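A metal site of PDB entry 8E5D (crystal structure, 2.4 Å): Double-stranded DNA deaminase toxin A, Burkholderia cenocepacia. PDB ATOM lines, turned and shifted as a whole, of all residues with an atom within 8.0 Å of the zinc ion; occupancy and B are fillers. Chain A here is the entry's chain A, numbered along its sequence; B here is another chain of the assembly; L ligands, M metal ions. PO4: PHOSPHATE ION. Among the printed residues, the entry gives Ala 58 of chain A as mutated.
NE2 of His 56 is in hydrogen-bond range of O2 of DT 7 of chain B (3.0 Å).
The backbone carbonyl oxygen (O) of Ala 52 sits at hydrogen-bond distance from a ring nitrogen (NE2) of His 56 (3.1 Å).
The side-chain hydroxyl (OG1) of Thr 91 is in hydrogen-bond range of the backbone carbonyl oxygen (O) of Cys 87, 2.8 Å away.
SG of Cys 84 lies close to N of Phe 86, 3.3 Å away.
O1 of the ligand is bound to the zinc ion (1.9 Å).
ND1 of His 56 is bound to the zinc ion (2.0 Å).
The zinc ion is bound by SG of Cys 87 (2.2 Å).
The side-chain sulfur (SG) of Cys 84 binds the zinc ion.
Of the 22 residues printed, 3 come within 4 Å of the zinc ion.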
ATOM      1  N   THR A  22      22.626   7.473 -21.149  1.00  0.00           N
ATOM      2  CA  THR A  22      22.817   8.908 -20.992  1.00  0.00           C
ATOM      3  C   THR A  22      22.192   9.398 -19.687  1.00  0.00           C
ATOM      4  O   THR A  22      21.085   8.985 -19.310  1.00  0.00           O
ATOM      5  CB  THR A  22      22.217   9.669 -22.171  1.00  0.00           C
ATOM      6  OG1 THR A  22      22.690   9.096 -23.403  1.00  0.00           O
ATOM      7  CG2 THR A  22      22.646  11.132 -22.126  1.00  0.00           C
ATOM      8  N   SER A  42      18.259   8.260 -18.866  1.00  0.00           N
ATOM      9  CA  SER A  42      17.531   7.931 -20.084  1.00  0.00           C
ATOM     10  C   SER A  42      16.858   6.568 -19.980  1.00  0.00           C
ATOM     11  O   SER A  42      17.428   5.596 -19.481  1.00  0.00           O
ATOM     12  CB  SER A  42      18.476   7.950 -21.291  1.00  0.00           C
ATOM     13  OG  SER A  42      19.545   7.044 -21.121  1.00  0.00           O
ATOM     14  N   ALA A  52      10.441   8.227 -30.250  1.00  0.00           N
ATOM     15  CA  ALA A  52      11.747   7.631 -30.015  1.00  0.00           C
ATOM     16  C   ALA A  52      12.638   8.483 -29.123  1.00  0.00           C
ATOM     17  O   ALA A  52      13.607   7.963 -28.559  1.00  0.00           O
ATOM     18  CB  ALA A  52      12.448   7.373 -31.346  1.00  0.00           C
ATOM     19  N   ASN A  53      12.364   9.785 -28.989  1.00  0.00           N
ATOM     20  CA  ASN A  53      13.168  10.665 -28.166  1.00  0.00           C
ATOM     21  C   ASN A  53      12.569  10.913 -26.795  1.00  0.00           C
ATOM     22  O   ASN A  53      13.202  11.577 -25.973  1.00  0.00           O
ATOM     23  CB  ASN A  53      13.389  12.009 -28.851  1.00  0.00           C
ATOM     24  CG  ASN A  53      12.111  12.839 -28.941  1.00  0.00           C
ATOM     25  OD1 ASN A  53      11.056  12.334 -29.289  1.00  0.00           O
ATOM     26  ND2 ASN A  53      12.219  14.130 -28.603  1.00  0.00           N
ATOM     27  N   ALA A  54      11.361  10.408 -26.534  1.00  0.00           N
ATOM     28  CA  ALA A  54      10.687  10.725 -25.261  1.00  0.00           C
ATOM     29  C   ALA A  54      11.488  10.214 -24.072  1.00  0.00           C
ATOM     30  O   ALA A  54      11.582  10.897 -23.052  1.00  0.00           O
ATOM     31  CB  ALA A  54       9.280  10.134 -25.267  1.00  0.00           C
ATOM     32  N   GLY A  55      12.070   9.024 -24.195  1.00  0.00           N
ATOM     33  CA  GLY A  55      12.813   8.436 -23.093  1.00  0.00           C
ATOM     34  C   GLY A  55      14.225   8.945 -22.916  1.00  0.00           C
ATOM     35  O   GLY A  55      14.872   8.585 -21.928  1.00  0.00           O
ATOM     36  N   HIS A  56      14.717   9.774 -23.837  1.00  0.00           N
ATOM     37  CA  HIS A  56      16.046  10.346 -23.702  1.00  0.00           C
ATOM     38  C   HIS A  56      16.048  11.454 -22.651  1.00  0.00           C
ATOM     39  O   HIS A  56      15.012  11.860 -22.134  1.00  0.00           O
ATOM     40  CB  HIS A  56      16.545  10.886 -25.035  1.00  0.00           C
ATOM     41  CG  HIS A  56      16.618   9.865 -26.128  1.00  0.00           C
ATOM     42  ND1 HIS A  56      17.355  10.064 -27.280  1.00  0.00           N
ATOM     43  CD2 HIS A  56      16.055   8.647 -26.251  1.00  0.00           C
ATOM     44  CE1 HIS A  56      17.231   9.016 -28.065  1.00  0.00           C
ATOM     45  NE2 HIS A  56      16.452   8.134 -27.463  1.00  0.00           N
ATOM     46  N   VAL A  57      17.249  11.961 -22.356  1.00  0.00           N
ATOM     47  CA  VAL A  57      17.396  13.005 -21.351  1.00  0.00           C
ATOM     48  C   VAL A  57      16.676  14.284 -21.790  1.00  0.00           C
ATOM     49  O   VAL A  57      15.917  14.897 -21.021  1.00  0.00           O
ATOM     50  CB  VAL A  57      18.883  13.258 -21.058  1.00  0.00           C
ATOM     51  CG1 VAL A  57      19.091  14.666 -20.552  1.00  0.00           C
ATOM     52  CG2 VAL A  57      19.401  12.259 -20.051  1.00  0.00           C
ATOM     53  N   ALA A  58      16.887  14.687 -23.040  1.00  0.00           N
ATOM     54  CA  ALA A  58      16.236  15.894 -23.526  1.00  0.00           C
ATOM     55  C   ALA A  58      14.727  15.697 -23.655  1.00  0.00           C
ATOM     56  O   ALA A  58      13.950  16.612 -23.382  1.00  0.00           O
ATOM     57  CB  ALA A  58      16.850  16.320 -24.865  1.00  0.00           C
ATOM     58  N   GLY A  59      14.303  14.492 -24.048  1.00  0.00           N
ATOM     59  CA  GLY A  59      12.876  14.212 -24.104  1.00  0.00           C
ATOM     60  C   GLY A  59      12.197  14.253 -22.746  1.00  0.00           C
ATOM     61  O   GLY A  59      11.114  14.840 -22.603  1.00  0.00           O
ATOM     62  N   HIS A  77      24.100  16.741 -20.578  1.00  0.00           N
ATOM     63  CA  HIS A  77      24.165  15.294 -20.585  1.00  0.00           C
ATOM     64  C   HIS A  77      25.602  14.849 -20.857  1.00  0.00           C
ATOM     65  O   HIS A  77      26.499  15.670 -21.095  1.00  0.00           O
ATOM     66  CB  HIS A  77      23.196  14.681 -21.598  1.00  0.00           C
ATOM     67  CG  HIS A  77      23.529  14.943 -23.034  1.00  0.00           C
ATOM     68  ND1 HIS A  77      24.396  14.154 -23.753  1.00  0.00           N
ATOM     69  CD2 HIS A  77      23.084  15.888 -23.893  1.00  0.00           C
ATOM     70  CE1 HIS A  77      24.492  14.605 -24.987  1.00  0.00           C
ATOM     71  NE2 HIS A  77      23.699  15.667 -25.102  1.00  0.00           N
ATOM     72  N   ASN A  79      26.751  12.168 -22.990  1.00  0.00           N
ATOM     73  CA  ASN A  79      26.943  11.269 -24.128  1.00  0.00           C
ATOM     74  C   ASN A  79      27.984  11.813 -25.101  1.00  0.00           C
ATOM     75  O   ASN A  79      27.743  12.833 -25.756  1.00  0.00           O
ATOM     76  CB  ASN A  79      25.613  11.061 -24.850  1.00  0.00           C
ATOM     77  CG  ASN A  79      25.647   9.898 -25.822  1.00  0.00           C
ATOM     78  OD1 ASN A  79      26.715   9.389 -26.183  1.00  0.00           O
ATOM     79  ND2 ASN A  79      24.470   9.475 -26.281  1.00  0.00           N
ATOM     80  N   GLY A  82      26.966  12.855 -28.590  1.00  0.00           N
ATOM     81  CA  GLY A  82      26.128  14.018 -28.756  1.00  0.00           C
ATOM     82  C   GLY A  82      24.636  13.740 -28.629  1.00  0.00           C
ATOM     83  O   GLY A  82      24.191  12.655 -28.267  1.00  0.00           O
ATOM     84  N   THR A  83      23.867  14.783 -28.917  1.00  0.00           N
ATOM     85  CA  THR A  83      22.418  14.698 -28.970  1.00  0.00           C
ATOM     86  C   THR A  83      21.995  14.049 -30.290  1.00  0.00           C
ATOM     87  O   THR A  83      22.474  14.447 -31.354  1.00  0.00           O
ATOM     88  CB  THR A  83      21.805  16.083 -28.837  1.00  0.00           C
ATOM     89  OG1 THR A  83      22.374  16.761 -27.707  1.00  0.00           O
ATOM     90  CG2 THR A  83      20.315  15.984 -28.639  1.00  0.00           C
ATOM     91  N   CYS A  84      21.110  13.059 -30.222  1.00  0.00           N
ATOM     92  CA  CYS A  84      20.790  12.239 -31.380  1.00  0.00           C
ATOM     93  C   CYS A  84      19.893  12.979 -32.374  1.00  0.00           C
ATOM     94  O   CYS A  84      19.470  14.117 -32.153  1.00  0.00           O
ATOM     95  CB  CYS A  84      20.126  10.938 -30.931  1.00  0.00           C
ATOM     96  SG  CYS A  84      18.350  11.095 -30.609  1.00  0.00           S
ATOM     97  N   GLY A  85      19.589  12.315 -33.495  1.00  0.00           N
ATOM     98  CA  GLY A  85      18.781  12.945 -34.528  1.00  0.00           C
ATOM     99  C   GLY A  85      17.298  12.988 -34.186  1.00  0.00           C
ATOM    100  O   GLY A  85      16.576  13.908 -34.609  1.00  0.00           O
ATOM    101  N   PHE A  86      16.819  12.005 -33.416  1.00  0.00           N
ATOM    102  CA  PHE A  86      15.426  12.044 -32.983  1.00  0.00           C
ATOM    103  C   PHE A  86      15.184  13.229 -32.060  1.00  0.00           C
ATOM    104  O   PHE A  86      14.166  13.921 -32.196  1.00  0.00           O
ATOM    105  CB  PHE A  86      15.047  10.747 -32.291  1.00  0.00           C
ATOM    106  CG  PHE A  86      15.045   9.557 -33.194  1.00  0.00           C
ATOM    107  CD1 PHE A  86      14.207   9.519 -34.297  1.00  0.00           C
ATOM    108  CD2 PHE A  86      15.857   8.462 -32.936  1.00  0.00           C
ATOM    109  CE1 PHE A  86      14.186   8.416 -35.133  1.00  0.00           C
ATOM    110  CE2 PHE A  86      15.845   7.359 -33.777  1.00  0.00           C
ATOM    111  CZ  PHE A  86      15.008   7.331 -34.877  1.00  0.00           C
ATOM    112  N   CYS A  87      16.098  13.481 -31.123  1.00  0.00           N
ATOM    113  CA  CYS A  87      15.966  14.661 -30.271  1.00  0.00           C
ATOM    114  C   CYS A  87      15.941  15.932 -31.116  1.00  0.00           C
ATOM    115  O   CYS A  87      15.015  16.754 -30.991  1.00  0.00           O
ATOM    116  CB  CYS A  87      17.102  14.715 -29.249  1.00  0.00           C
ATOM    117  SG  CYS A  87      17.033  13.408 -28.005  1.00  0.00           S
ATOM    118  N   VAL A  88      16.925  16.069 -32.000  1.00  0.00           N
ATOM    119  CA  VAL A  88      17.051  17.261 -32.848  1.00  0.00           C
ATOM    120  C   VAL A  88      15.760  17.527 -33.627  1.00  0.00           C
ATOM    121  O   VAL A  88      15.376  18.675 -33.833  1.00  0.00           O
ATOM    122  CB  VAL A  88      18.258  17.116 -33.808  1.00  0.00           C
ATOM    123  CG1 VAL A  88      18.286  18.241 -34.816  1.00  0.00           C
ATOM    124  CG2 VAL A  88      19.557  17.117 -33.028  1.00  0.00           C
ATOM    125  N   THR A  91      12.108  17.327 -30.319  1.00  0.00           N
ATOM    126  CA  THR A  91      11.971  18.021 -29.053  1.00  0.00           C
ATOM    127  C   THR A  91      10.977  19.177 -29.147  1.00  0.00           C
ATOM    128  O   THR A  91      10.155  19.380 -28.246  1.00  0.00           O
ATOM    129  CB  THR A  91      13.337  18.508 -28.598  1.00  0.00           C
ATOM    130  OG1 THR A  91      14.165  17.369 -28.373  1.00  0.00           O
ATOM    131  CG2 THR A  91      13.218  19.317 -27.332  1.00  0.00           C
ATOM    132  P    DT B   7      20.683   5.517 -33.988  1.00  0.00           P
ATOM    133  OP1  DT B   7      21.910   4.713 -33.794  1.00  0.00           O
ATOM    134  OP2  DT B   7      19.383   4.825 -34.163  1.00  0.00           O
ATOM    135  O5'  DT B   7      20.602   6.486 -32.740  1.00  0.00           O
ATOM    136  C5'  DT B   7      19.357   6.914 -32.271  1.00  0.00           C
ATOM    137  C4'  DT B   7      19.326   6.807 -30.760  1.00  0.00           C
ATOM    138  O4'  DT B   7      17.949   6.717 -30.335  1.00  0.00           O
ATOM    139  C3'  DT B   7      20.001   5.557 -30.193  1.00  0.00           C
ATOM    140  O3'  DT B   7      20.467   5.836 -28.882  1.00  0.00           O
ATOM    141  C2'  DT B   7      18.839   4.563 -30.187  1.00  0.00           C
ATOM    142  C1'  DT B   7      17.728   5.469 -29.710  1.00  0.00           C
ATOM    143  N1   DT B   7      16.352   5.031 -30.054  1.00  0.00           N
ATOM    144  C2   DT B   7      15.417   4.976 -29.059  1.00  0.00           C
ATOM    145  O2   DT B   7      15.671   5.231 -27.909  1.00  0.00           O
ATOM    146  N3   DT B   7      14.171   4.598 -29.458  1.00  0.00           N
ATOM    147  C4   DT B   7      13.757   4.275 -30.735  1.00  0.00           C
ATOM    148  O4   DT B   7      12.613   3.946 -30.986  1.00  0.00           O
ATOM    149  C5   DT B   7      14.784   4.375 -31.750  1.00  0.00           C
ATOM    150  C7   DT B   7      14.466   4.068 -33.185  1.00  0.00           C
ATOM    151  C6   DT B   7      16.018   4.751 -31.370  1.00  0.00           C
ATOM    152  P    DC B   8      21.885   5.289 -28.347  1.00  0.00           P
ATOM    153  OP1  DC B   8      22.602   6.437 -27.757  1.00  0.00           O
ATOM    154  OP2  DC B   8      22.530   4.497 -29.410  1.00  0.00           O
ATOM    155  O5'  DC B   8      21.474   4.273 -27.175  1.00  0.00           O
ATOM    156  C5'  DC B   8      20.488   4.656 -26.212  1.00  0.00           C
ATOM    157  C4'  DC B   8      19.749   3.439 -25.653  1.00  0.00           C
ATOM    158  O4'  DC B   8      19.285   2.598 -26.739  1.00  0.00           O
ATOM    159  C3'  DC B   8      20.563   2.552 -24.721  1.00  0.00           C
ATOM    160  O3'  DC B   8      19.771   2.172 -23.574  1.00  0.00           O
ATOM    161  C2'  DC B   8      20.908   1.340 -25.588  1.00  0.00           C
ATOM    162  C1'  DC B   8      19.705   1.265 -26.516  1.00  0.00           C
ATOM    163  N1   DC B   8      20.005   0.674 -27.854  1.00  0.00           N
ATOM    164  C2   DC B   8      19.558  -0.619 -28.166  1.00  0.00           C
ATOM    165  O2   DC B   8      18.918  -1.268 -27.315  1.00  0.00           O
ATOM    166  N3   DC B   8      19.842  -1.126 -29.398  1.00  0.00           N
ATOM    167  C4   DC B   8      20.536  -0.388 -30.287  1.00  0.00           C
ATOM    168  N4   DC B   8      20.787  -0.923 -31.481  1.00  0.00           N
ATOM    169  C5   DC B   8      20.989   0.928 -29.981  1.00  0.00           C
ATOM    170  C6   DC B   8      20.704   1.420 -28.769  1.00  0.00           C
HETATM  171  P   PO4 L   1      20.836  10.703 -26.664  1.00  0.00           P
HETATM  172  O1  PO4 L   1      20.078  11.246 -27.843  1.00  0.00           O
HETATM  173  O2  PO4 L   1      19.984  10.695 -25.413  1.00  0.00           O
HETATM  174  O3  PO4 L   1      21.264   9.295 -27.004  1.00  0.00           O
HETATM  175  O4  PO4 L   1      22.056  11.561 -26.430  1.00  0.00           O
HETATM  176 ZN    ZN M   1      18.225  11.542 -28.320  1.00  0.00          ZN
